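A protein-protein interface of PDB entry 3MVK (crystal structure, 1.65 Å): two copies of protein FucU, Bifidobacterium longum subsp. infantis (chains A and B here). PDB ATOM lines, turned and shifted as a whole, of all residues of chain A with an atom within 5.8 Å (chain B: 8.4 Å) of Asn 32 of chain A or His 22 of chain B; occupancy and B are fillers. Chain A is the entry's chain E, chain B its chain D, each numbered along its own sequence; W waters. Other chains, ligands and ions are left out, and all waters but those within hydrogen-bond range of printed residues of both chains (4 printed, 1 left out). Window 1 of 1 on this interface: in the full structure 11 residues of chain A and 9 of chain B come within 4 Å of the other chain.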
ATOM      1  N   ASP A  30      22.818  37.521   5.521  1.00  0.00           N
ATOM      2  CA  ASP A  30      23.729  36.685   4.740  1.00  0.00           C
ATOM      3  C   ASP A  30      23.027  35.987   3.569  1.00  0.00           C
ATOM      4  O   ASP A  30      21.805  36.092   3.403  1.00  0.00           O
ATOM      5  CB  ASP A  30      24.560  35.733   5.648  1.00  0.00           C
ATOM      6  CG  ASP A  30      23.752  34.590   6.254  1.00  0.00           C
ATOM      7  OD1 ASP A  30      22.712  34.188   5.700  1.00  0.00           O
ATOM      8  OD2 ASP A  30      24.188  34.046   7.310  1.00  0.00           O
ATOM      9  N   GLY A  31      23.798  35.334   2.712  1.00  0.00           N
ATOM     10  CA  GLY A  31      23.252  34.820   1.451  1.00  0.00           C
ATOM     11  C   GLY A  31      22.243  33.709   1.660  1.00  0.00           C
ATOM     12  O   GLY A  31      21.410  33.437   0.781  1.00  0.00           O
ATOM     13  N   ASN A  32      22.313  33.065   2.816  1.00  0.00           N
ATOM     14  CA  ASN A  32      21.364  32.013   3.148  1.00  0.00           C
ATOM     15  C   ASN A  32      20.087  32.467   3.856  1.00  0.00           C
ATOM     16  O   ASN A  32      19.173  31.669   4.073  1.00  0.00           O
ATOM     17  CB  ASN A  32      22.060  30.964   3.997  1.00  0.00           C
ATOM     18  CG  ASN A  32      22.801  29.964   3.130  1.00  0.00           C
ATOM     19  OD1 ASN A  32      22.179  29.177   2.434  1.00  0.00           O
ATOM     20  ND2 ASN A  32      24.099  30.018   3.141  1.00  0.00           N
ATOM     21  N   PHE A  33      20.031  33.743   4.213  1.00  0.00           N
ATOM     22  CA  PHE A  33      18.953  34.257   5.047  1.00  0.00           C
ATOM     23  C   PHE A  33      17.694  34.442   4.197  1.00  0.00           C
ATOM     24  O   PHE A  33      17.793  34.830   3.039  1.00  0.00           O
ATOM     25  CB  PHE A  33      19.394  35.611   5.632  1.00  0.00           C
ATOM     26  CG  PHE A  33      18.488  36.151   6.708  1.00  0.00           C
ATOM     27  CD1 PHE A  33      18.579  35.694   8.025  1.00  0.00           C
ATOM     28  CD2 PHE A  33      17.546  37.123   6.398  1.00  0.00           C
ATOM     29  CE1 PHE A  33      17.747  36.199   9.033  1.00  0.00           C
ATOM     30  CE2 PHE A  33      16.704  37.644   7.394  1.00  0.00           C
ATOM     31  CZ  PHE A  33      16.803  37.204   8.716  1.00  0.00           C
ATOM     32  N   PRO A  34      16.520  34.196   4.773  1.00  0.00           N
ATOM     33  CA  PRO A  34      15.256  34.413   4.020  1.00  0.00           C
ATOM     34  C   PRO A  34      14.894  35.902   4.036  1.00  0.00           C
ATOM     35  O   PRO A  34      13.951  36.311   4.724  1.00  0.00           O
ATOM     36  CB  PRO A  34      14.242  33.577   4.795  1.00  0.00           C
ATOM     37  CG  PRO A  34      14.824  33.475   6.224  1.00  0.00           C
ATOM     38  CD  PRO A  34      16.308  33.505   6.061  1.00  0.00           C
ATOM     39  N   ARG A 112      18.400  31.382  16.983  1.00  0.00           N
ATOM     40  CA  ARG A 112      17.960  31.479  15.577  1.00  0.00           C
ATOM     41  C   ARG A 112      16.522  31.967  15.383  1.00  0.00           C
ATOM     42  O   ARG A 112      16.274  32.949  14.660  1.00  0.00           O
ATOM     43  CB  ARG A 112      18.147  30.116  14.866  1.00  0.00           C
ATOM     44  CG  ARG A 112      17.626  30.119  13.436  1.00  0.00           C
ATOM     45  CD  ARG A 112      18.067  28.893  12.634  1.00  0.00           C
ATOM     46  NE  ARG A 112      17.426  28.936  11.323  1.00  0.00           N
ATOM     47  CZ  ARG A 112      16.925  27.897  10.658  1.00  0.00           C
ATOM     48  NH1 ARG A 112      17.001  26.649  11.141  1.00  0.00           N
ATOM     49  NH2 ARG A 112      16.360  28.117   9.471  1.00  0.00           N
ATOM     50  N   TYR A 116      14.998  35.569  13.989  1.00  0.00           N
ATOM     51  CA  TYR A 116      14.003  35.771  12.919  1.00  0.00           C
ATOM     52  C   TYR A 116      12.876  36.697  13.375  1.00  0.00           C
ATOM     53  O   TYR A 116      12.457  37.584  12.632  1.00  0.00           O
ATOM     54  CB  TYR A 116      13.395  34.453  12.424  1.00  0.00           C
ATOM     55  CG  TYR A 116      14.320  33.571  11.614  1.00  0.00           C
ATOM     56  CD1 TYR A 116      15.208  34.117  10.686  1.00  0.00           C
ATOM     57  CD2 TYR A 116      14.278  32.180  11.767  1.00  0.00           C
ATOM     58  CE1 TYR A 116      16.049  33.312   9.929  1.00  0.00           C
ATOM     59  CE2 TYR A 116      15.118  31.366  11.026  1.00  0.00           C
ATOM     60  CZ  TYR A 116      15.995  31.937  10.106  1.00  0.00           C
ATOM     61  OH  TYR A 116      16.816  31.119   9.375  1.00  0.00           O
ATOM     62  N   GLU A 130      26.698  37.239   1.168  1.00  0.00           N
ATOM     63  CA  GLU A 130      27.706  36.684   2.092  1.00  0.00           C
ATOM     64  C   GLU A 130      27.576  35.158   2.160  1.00  0.00           C
ATOM     65  O   GLU A 130      26.515  34.626   2.489  1.00  0.00           O
ATOM     66  CB  GLU A 130      27.544  37.316   3.486  1.00  0.00           C
ATOM     67  CG  GLU A 130      28.566  36.818   4.544  1.00  0.00           C
ATOM     68  CD  GLU A 130      29.988  36.815   4.001  1.00  0.00           C
ATOM     69  OE1 GLU A 130      30.479  37.883   3.563  1.00  0.00           O
ATOM     70  OE2 GLU A 130      30.624  35.737   4.002  1.00  0.00           O
ATOM     71  N   SER A 131      28.655  34.451   1.829  1.00  0.00           N
ATOM     72  CA  SER A 131      28.592  32.986   1.808  1.00  0.00           C
ATOM     73  C   SER A 131      28.794  32.306   3.180  1.00  0.00           C
ATOM     74  O   SER A 131      28.371  31.161   3.369  1.00  0.00           O
ATOM     75  CB  SER A 131      29.571  32.434   0.753  1.00  0.00           C
ATOM     76  OG  SER A 131      30.910  32.700   1.125  1.00  0.00           O
ATOM     77  N   ALA A 132      29.421  33.004   4.122  1.00  0.00           N
ATOM     78  CA  ALA A 132      29.574  32.486   5.493  1.00  0.00           C
ATOM     79  C   ALA A 132      28.214  32.278   6.144  1.00  0.00           C
ATOM     80  O   ALA A 132      27.324  33.120   6.008  1.00  0.00           O
ATOM     81  CB  ALA A 132      30.396  33.422   6.313  1.00  0.00           C
ATOM     82  N   GLN A 133      28.049  31.142   6.827  1.00  0.00           N
ATOM     83  CA  GLN A 133      26.883  30.925   7.671  1.00  0.00           C
ATOM     84  C   GLN A 133      26.950  31.760   8.956  1.00  0.00           C
ATOM     85  O   GLN A 133      28.035  32.124   9.440  1.00  0.00           O
ATOM     86  CB  GLN A 133      26.716  29.443   8.019  1.00  0.00           C
ATOM     87  CG  GLN A 133      25.857  28.678   7.005  1.00  0.00           C
ATOM     88  CD  GLN A 133      25.563  27.277   7.487  1.00  0.00           C
ATOM     89  OE1 GLN A 133      26.464  26.447   7.576  1.00  0.00           O
ATOM     90  NE2 GLN A 133      24.304  27.017   7.834  1.00  0.00           N
ATOM     91  N   CYS B  18      15.108  31.640  -6.091  1.00  0.00           N
ATOM     92  CA  CYS B  18      16.373  32.282  -5.747  1.00  0.00           C
ATOM     93  C   CYS B  18      16.272  33.177  -4.518  1.00  0.00           C
ATOM     94  O   CYS B  18      17.205  33.223  -3.700  1.00  0.00           O
ATOM     95  CB  CYS B  18      16.914  33.071  -6.945  1.00  0.00           C
ATOM     96  SG  CYS B  18      17.471  32.015  -8.285  1.00  0.00           S
ATOM     97  N   GLU B  19      15.155  33.876  -4.367  1.00  0.00           N
ATOM     98  CA  GLU B  19      14.997  34.773  -3.226  1.00  0.00           C
ATOM     99  C   GLU B  19      14.549  34.087  -1.916  1.00  0.00           C
ATOM    100  O   GLU B  19      14.624  34.684  -0.830  1.00  0.00           O
ATOM    101  CB  GLU B  19      14.102  35.944  -3.581  1.00  0.00           C
ATOM    102  CG  GLU B  19      12.677  35.615  -3.627  1.00  0.00           C
ATOM    103  CD  GLU B  19      11.879  36.638  -4.412  1.00  0.00           C
ATOM    104  OE1 GLU B  19      12.466  37.596  -4.955  1.00  0.00           O
ATOM    105  OE2 GLU B  19      10.659  36.483  -4.482  1.00  0.00           O
ATOM    106  N   MET B  20      14.069  32.856  -2.020  1.00  0.00           N
ATOM    107  CA  MET B  20      13.828  32.070  -0.810  1.00  0.00           C
ATOM    108  C   MET B  20      15.145  31.771  -0.111  1.00  0.00           C
ATOM    109  O   MET B  20      16.170  31.543  -0.767  1.00  0.00           O
ATOM    110  CB  MET B  20      13.089  30.766  -1.130  1.00  0.00           C
ATOM    111  CG  MET B  20      11.610  31.026  -1.442  1.00  0.00           C
ATOM    112  SD  MET B  20      10.715  29.463  -2.191  1.00  0.00           S
ATOM    113  CE  MET B  20      10.678  28.360  -0.541  1.00  0.00           C
ATOM    114  N   GLY B  21      15.081  31.708   1.210  1.00  0.00           N
ATOM    115  CA  GLY B  21      16.263  31.454   2.030  1.00  0.00           C
ATOM    116  C   GLY B  21      15.995  30.284   2.965  1.00  0.00           C
ATOM    117  O   GLY B  21      14.973  29.615   2.872  1.00  0.00           O
ATOM    118  N   HIS B  22      16.929  30.065   3.888  1.00  0.00           N
ATOM    119  CA  HIS B  22      16.918  28.884   4.750  1.00  0.00           C
ATOM    120  C   HIS B  22      15.694  28.872   5.631  1.00  0.00           C
ATOM    121  O   HIS B  22      15.464  29.815   6.401  1.00  0.00           O
ATOM    122  CB  HIS B  22      18.194  28.889   5.612  1.00  0.00           C
ATOM    123  CG  HIS B  22      18.362  27.655   6.438  1.00  0.00           C
ATOM    124  ND1 HIS B  22      19.189  27.610   7.543  1.00  0.00           N
ATOM    125  CD2 HIS B  22      17.836  26.413   6.300  1.00  0.00           C
ATOM    126  CE1 HIS B  22      19.159  26.388   8.056  1.00  0.00           C
ATOM    127  NE2 HIS B  22      18.347  25.645   7.320  1.00  0.00           N
ATOM    128  N   GLY B  23      14.879  27.824   5.492  1.00  0.00           N
ATOM    129  CA  GLY B  23      13.636  27.702   6.246  1.00  0.00           C
ATOM    130  C   GLY B  23      12.356  28.127   5.543  1.00  0.00           C
ATOM    131  O   GLY B  23      11.249  27.784   5.988  1.00  0.00           O
ATOM    132  N   ASP B  24      12.490  28.870   4.447  1.00  0.00           N
ATOM    133  CA  ASP B  24      11.318  29.249   3.661  1.00  0.00           C
ATOM    134  C   ASP B  24      10.665  28.004   3.072  1.00  0.00           C
ATOM    135  O   ASP B  24      11.325  27.014   2.742  1.00  0.00           O
ATOM    136  CB  ASP B  24      11.695  30.193   2.519  1.00  0.00           C
ATOM    137  CG  ASP B  24      11.789  31.640   2.946  1.00  0.00           C
ATOM    138  OD1 ASP B  24      11.100  32.067   3.900  1.00  0.00           O
ATOM    139  OD2 ASP B  24      12.553  32.373   2.291  1.00  0.00           O
ATOM    140  N   GLN B  25       9.357  28.059   2.927  1.00  0.00           N
ATOM    141  CA  GLN B  25       8.629  26.925   2.388  1.00  0.00           C
ATOM    142  C   GLN B  25       7.883  27.260   1.102  1.00  0.00           C
ATOM    143  O   GLN B  25       7.415  28.386   0.890  1.00  0.00           O
ATOM    144  CB  GLN B  25       7.647  26.381   3.429  1.00  0.00           C
ATOM    145  CG  GLN B  25       8.328  25.694   4.620  1.00  0.00           C
ATOM    146  CD  GLN B  25       7.339  25.131   5.615  1.00  0.00           C
ATOM    147  OE1 GLN B  25       6.136  25.373   5.531  1.00  0.00           O
ATOM    148  NE2 GLN B  25       7.848  24.362   6.567  1.00  0.00           N
ATOM    149  N   PHE B  63      16.941  23.683  -5.847  1.00  0.00           N
ATOM    150  CA  PHE B  63      16.423  23.963  -4.503  1.00  0.00           C
ATOM    151  C   PHE B  63      16.886  22.870  -3.545  1.00  0.00           C
ATOM    152  O   PHE B  63      16.467  21.718  -3.663  1.00  0.00           O
ATOM    153  CB  PHE B  63      14.898  23.981  -4.621  1.00  0.00           C
ATOM    154  CG  PHE B  63      14.137  24.368  -3.380  1.00  0.00           C
ATOM    155  CD1 PHE B  63      13.660  25.672  -3.236  1.00  0.00           C
ATOM    156  CD2 PHE B  63      13.773  23.420  -2.441  1.00  0.00           C
ATOM    157  CE1 PHE B  63      12.865  26.017  -2.135  1.00  0.00           C
ATOM    158  CE2 PHE B  63      12.987  23.756  -1.334  1.00  0.00           C
ATOM    159  CZ  PHE B  63      12.528  25.060  -1.198  1.00  0.00           C
ATOM    160  N   PRO B  64      17.779  23.213  -2.605  1.00  0.00           N
ATOM    161  CA  PRO B  64      18.218  22.212  -1.627  1.00  0.00           C
ATOM    162  C   PRO B  64      17.182  22.004  -0.524  1.00  0.00           C
ATOM    163  O   PRO B  64      16.625  22.974  -0.027  1.00  0.00           O
ATOM    164  CB  PRO B  64      19.490  22.841  -1.047  1.00  0.00           C
ATOM    165  CG  PRO B  64      19.250  24.321  -1.145  1.00  0.00           C
ATOM    166  CD  PRO B  64      18.369  24.543  -2.352  1.00  0.00           C
ATOM    167  N   LEU B  65      16.931  20.760  -0.127  1.00  0.00           N
ATOM    168  CA  LEU B  65      15.982  20.511   0.951  1.00  0.00           C
ATOM    169  C   LEU B  65      16.680  20.643   2.297  1.00  0.00           C
ATOM    170  O   LEU B  65      17.806  20.164   2.479  1.00  0.00           O
ATOM    171  CB  LEU B  65      15.339  19.136   0.829  1.00  0.00           C
ATOM    172  CG  LEU B  65      14.418  18.831  -0.345  1.00  0.00           C
ATOM    173  CD1 LEU B  65      13.981  17.356  -0.278  1.00  0.00           C
ATOM    174  CD2 LEU B  65      13.212  19.755  -0.333  1.00  0.00           C
ATOM    175  N   ASP B  66      16.013  21.295   3.241  1.00  0.00           N
ATOM    176  CA  ASP B  66      16.616  21.608   4.541  1.00  0.00           C
ATOM    177  C   ASP B  66      17.168  20.374   5.275  1.00  0.00           C
ATOM    178  O   ASP B  66      16.479  19.364   5.398  1.00  0.00           O
ATOM    179  CB  ASP B  66      15.581  22.314   5.412  1.00  0.00           C
ATOM    180  CG  ASP B  66      16.192  23.143   6.510  1.00  0.00           C
ATOM    181  OD1 ASP B  66      17.441  23.127   6.721  1.00  0.00           O
ATOM    182  OD2 ASP B  66      15.387  23.842   7.157  1.00  0.00           O
ATOM    183  N   THR B  67      18.420  20.452   5.714  1.00  0.00           N
ATOM    184  CA  THR B  67      19.004  19.380   6.544  1.00  0.00           C
ATOM    185  C   THR B  67      18.871  19.690   8.029  1.00  0.00           C
ATOM    186  O   THR B  67      19.261  18.871   8.878  1.00  0.00           O
ATOM    187  CB  THR B  67      20.497  19.113   6.219  1.00  0.00           C
ATOM    188  OG1 THR B  67      21.247  20.310   6.447  1.00  0.00           O
ATOM    189  CG2 THR B  67      20.677  18.673   4.777  1.00  0.00           C
ATOM    190  N   TYR B  68      18.320  20.860   8.367  1.00  0.00           N
ATOM    191  CA  TYR B  68      18.204  21.274   9.766  1.00  0.00           C
ATOM    192  C   TYR B  68      16.905  20.786  10.388  1.00  0.00           C
ATOM    193  O   TYR B  68      16.631  21.036  11.560  1.00  0.00           O
ATOM    194  CB  TYR B  68      18.312  22.802   9.894  1.00  0.00           C
ATOM    195  CG  TYR B  68      19.722  23.319   9.763  1.00  0.00           C
ATOM    196  CD1 TYR B  68      20.417  23.222   8.567  1.00  0.00           C
ATOM    197  CD2 TYR B  68      20.366  23.908  10.853  1.00  0.00           C
ATOM    198  CE1 TYR B  68      21.729  23.685   8.443  1.00  0.00           C
ATOM    199  CE2 TYR B  68      21.681  24.373  10.736  1.00  0.00           C
ATOM    200  CZ  TYR B  68      22.347  24.258   9.530  1.00  0.00           C
ATOM    201  OH  TYR B  68      23.639  24.706   9.414  1.00  0.00           O
ATOM    202  N   VAL B  69      16.089  20.116   9.582  1.00  0.00           N
ATOM    203  CA  VAL B  69      14.936  19.377  10.074  1.00  0.00           C
ATOM    204  C   VAL B  69      15.051  17.965   9.491  1.00  0.00           C
ATOM    205  O   VAL B  69      15.690  17.767   8.446  1.00  0.00           O
ATOM    206  CB  VAL B  69      13.594  20.062   9.682  1.00  0.00           C
ATOM    207  CG1 VAL B  69      13.493  21.438  10.322  1.00  0.00           C
ATOM    208  CG2 VAL B  69      13.423  20.134   8.158  1.00  0.00           C
ATOM    209  N   GLN B 140      10.710  22.593   2.298  1.00  0.00           N
ATOM    210  CA  GLN B 140      11.407  23.606   3.109  1.00  0.00           C
ATOM    211  C   GLN B 140      12.847  23.730   2.616  1.00  0.00           C
ATOM    212  O   GLN B 140      13.589  22.743   2.554  1.00  0.00           O
ATOM    213  CB  GLN B 140      11.390  23.212   4.593  1.00  0.00           C
ATOM    214  CG  GLN B 140      12.066  24.251   5.507  1.00  0.00           C
ATOM    215  CD  GLN B 140      11.683  24.043   6.944  1.00  0.00           C
ATOM    216  OE1 GLN B 140      10.500  24.017   7.281  1.00  0.00           O
ATOM    217  NE2 GLN B 140      12.679  23.921   7.812  1.00  0.00           N
ATOM    218  N   LYS B 141      13.244  24.950   2.270  1.00  0.00           N
ATOM    219  CA  LYS B 141      14.561  25.200   1.700  1.00  0.00           C
ATOM    220  C   LYS B 141      15.680  25.094   2.725  1.00  0.00           C
ATOM    221  O   LYS B 141      15.552  25.572   3.858  1.00  0.00           O
ATOM    222  CB  LYS B 141      14.606  26.599   1.072  1.00  0.00           C
ATOM    223  CG  LYS B 141      15.817  26.765   0.163  1.00  0.00           C
ATOM    224  CD  LYS B 141      15.813  28.100  -0.573  1.00  0.00           C
ATOM    225  CE  LYS B 141      17.063  28.277  -1.444  1.00  0.00           C
ATOM    226  NZ  LYS B 141      16.953  29.429  -2.408  1.00  0.00           N
ATOM    227  N   GLY B 142      16.773  24.455   2.318  1.00  0.00           N
ATOM    228  CA  GLY B 142      17.969  24.386   3.142  1.00  0.00           C
ATOM    229  C   GLY B 142      19.024  25.411   2.794  1.00  0.00           C
ATOM    230  O   GLY B 142      18.741  26.439   2.175  1.00  0.00           O
ATOM    231  N   VAL B 143      20.252  25.119   3.223  1.00  0.00           N
ATOM    232  CA  VAL B 143      21.367  26.027   3.066  1.00  0.00           C
ATOM    233  C   VAL B 143      22.089  25.729   1.767  1.00  0.00           C
ATOM    234  O   VAL B 143      22.195  24.568   1.343  1.00  0.00           O
ATOM    235  CB  VAL B 143      22.340  25.872   4.285  1.00  0.00           C
ATOM    236  CG1 VAL B 143      23.711  26.465   4.023  1.00  0.00           C
ATOM    237  CG2 VAL B 143      21.700  26.508   5.530  1.00  0.00           C
ATOM    238  N   VAL B 144      22.604  26.787   1.156  1.00  0.00           N
ATOM    239  CA  VAL B 144      23.609  26.656   0.110  1.00  0.00           C
ATOM    240  C   VAL B 144      24.971  26.906   0.776  1.00  0.00           C
ATOM    241  O   VAL B 144      25.219  28.004   1.268  1.00  0.00           O
ATOM    242  CB  VAL B 144      23.348  27.657  -1.018  1.00  0.00           C
ATOM    243  CG1 VAL B 144      24.421  27.524  -2.110  1.00  0.00           C
ATOM    244  CG2 VAL B 144      21.944  27.451  -1.595  1.00  0.00           C
ATOM    245  N   PHE B 145      25.832  25.878   0.805  1.00  0.00           N
ATOM    246  CA  PHE B 145      27.091  25.901   1.593  1.00  0.00           C
ATOM    247  C   PHE B 145      28.271  26.533   0.842  1.00  0.00           C
ATOM    248  O   PHE B 145      28.468  26.278  -0.352  1.00  0.00           O
ATOM    249  CB  PHE B 145      27.467  24.483   2.086  1.00  0.00           C
ATOM    250  CG  PHE B 145      26.520  23.919   3.121  1.00  0.00           C
ATOM    251  CD1 PHE B 145      26.662  24.245   4.472  1.00  0.00           C
ATOM    252  CD2 PHE B 145      25.484  23.063   2.747  1.00  0.00           C
ATOM    253  CE1 PHE B 145      25.782  23.728   5.441  1.00  0.00           C
ATOM    254  CE2 PHE B 145      24.593  22.533   3.708  1.00  0.00           C
ATOM    255  CZ  PHE B 145      24.741  22.871   5.059  1.00  0.00           C
HETATM  256  O   HOH W   1      26.917  24.237   9.156  1.00  0.00           O
HETATM  257  O   HOH W   2      15.430  25.391   9.236  1.00  0.00           O
HETATM  258  O   HOH W   3      26.795  30.051   1.018  1.00  0.00           O
HETATM  259  O   HOH W   4      19.319  29.125   1.620  1.00  0.00           O
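Among the printed residues, pairs that only touch across the chains: Asn 32 of chain A with Gly 21 of chain B, Asn 32 of chain A with Val 143 of chain B, Phe 33 of chain A with Gly 21 of chain B, Pro 34 of chain A with Gly 21 of chain B, Pro 34 of chain A with His 22 of chain B, Pro 34 of chain A with Asp 24 of chain B, Tyr 116 of chain A with His 22 of chain B, Gln 133 of chain A with Val 143 of chain B and Gln 133 of chain A with Phe 145 of chain B.
N of Tyr 68 of chain B sits at hydrogen-bond distance from OD1 of Asp 66 of chain B.
A ring nitrogen (NE2) of His 22 of chain B is in hydrogen-bond range of the side-chain carboxylate (OD1) of Asp 66 of chain B.
The side-chain carboxylate (OD1) of Asp 30 of chain A sits at hydrogen-bond distance from the backbone NH (N) of Phe 33 of chain A, 3.1 Å away.
The backbone NH (N) of Asn 32 of chain A lies close to the side-chain carboxylate (OD1) of Asp 30 of chain A (3.1 Å).
N of Gly 21 of chain B sits at hydrogen-bond distance from OD2 of Asp 24 of chain B (2.8 Å).
N of Lys 141 of chain B lies within hydrogen-bond range of O of Asp 24 of chain B (2.9 Å).
N of Val 144 of chain B sits at hydrogen-bond distance from OD1 of Asn 32 of chain A, at 2.7 Å.
OH of Tyr 68 of chain B is in hydrogen-bond range of NE2 of Gln 133 of chain A (2.9 Å).
O of Asn 32 of chain A lies within hydrogen-bond range of N of His 22 of chain B (2.8 Å).
A ring nitrogen (ND1) of His 22 of chain B is in hydrogen-bond range of the guanidinium group (NH2) of Arg 112 of chain A (3.5 Å).
No position is printed for both chains.
Water W2 lies within hydrogen-bond range of OD2 of Asp 66 of chain B (2.6 Å), NH1 of Arg 112 of chain A (2.8 Å), NE2 of Gln 140 of chain B (3.4 Å) and NE2 of His 22 of chain B (3.5 Å).
Water W3 lies within hydrogen-bond range of the backbone carbonyl oxygen (O) of Val 144 of chain B (2.6 Å), the backbone carbonyl oxygen (O) of Ser 131 of chain A (3.0 Å) and the side-chain amide nitrogen (ND2) of Asn 32 of chain A (3.4 Å).
Water W1 lies within hydrogen-bond range of OE1 of Gln 133 of chain A (2.8 Å) and OH of Tyr 68 of chain B (3.3 Å).
Water W4 lies within hydrogen-bond range of the backbone carbonyl oxygen of Gly 142 of chain B (2.8 Å), the side-chain amide oxygen of Asn 32 of chain A (3.0 Å) and the backbone NH of His 22 of chain B (3.4 Å).
Printed residues of chain B that touch a printed residue of chain A: Gly 21, His 22, Asp 24, Tyr 68, Val 143, Val 144 and Phe 145.
Hydrophobic or aromatic side chains of chain B that line the printed part of chain A: His 22, Tyr 68, Val 143, Val 144 and Phe 145.
Of the 11 printed residues of chain A, 6 touch a printed residue of chain B.
Printed residues of chain A that touch a printed residue of chain B: Asn 32, Phe 33, Pro 34, Arg 112, Tyr 116 and Gln 133.
Among the printed residues, no Asp or Glu carboxylate lies within 4 Å of a Lys or Arg side-chain nitrogen of the other chain.
No residue of chain B comes within 4 Å of Gly 31 of chain A.
Of chain A, only Asn 32, Pro 34, Arg 112 and Tyr 116 come within 4 Å of His 22 of chain B.
Of the printed residues of chain A, Tyr 68 of chain B touches Gln 133 (2.9 Å).
Printed residues of chain A within 4 Å of Val 144 of chain B: Asn 32 (2.7 Å).
The nearest residue of chain B that does not touch Asn 32 of chain A is Gly 142 of chain B (4.4 Å).
The nearest residue of chain A that does not touch His 22 of chain B is Phe 33 of chain A (4.5 Å).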
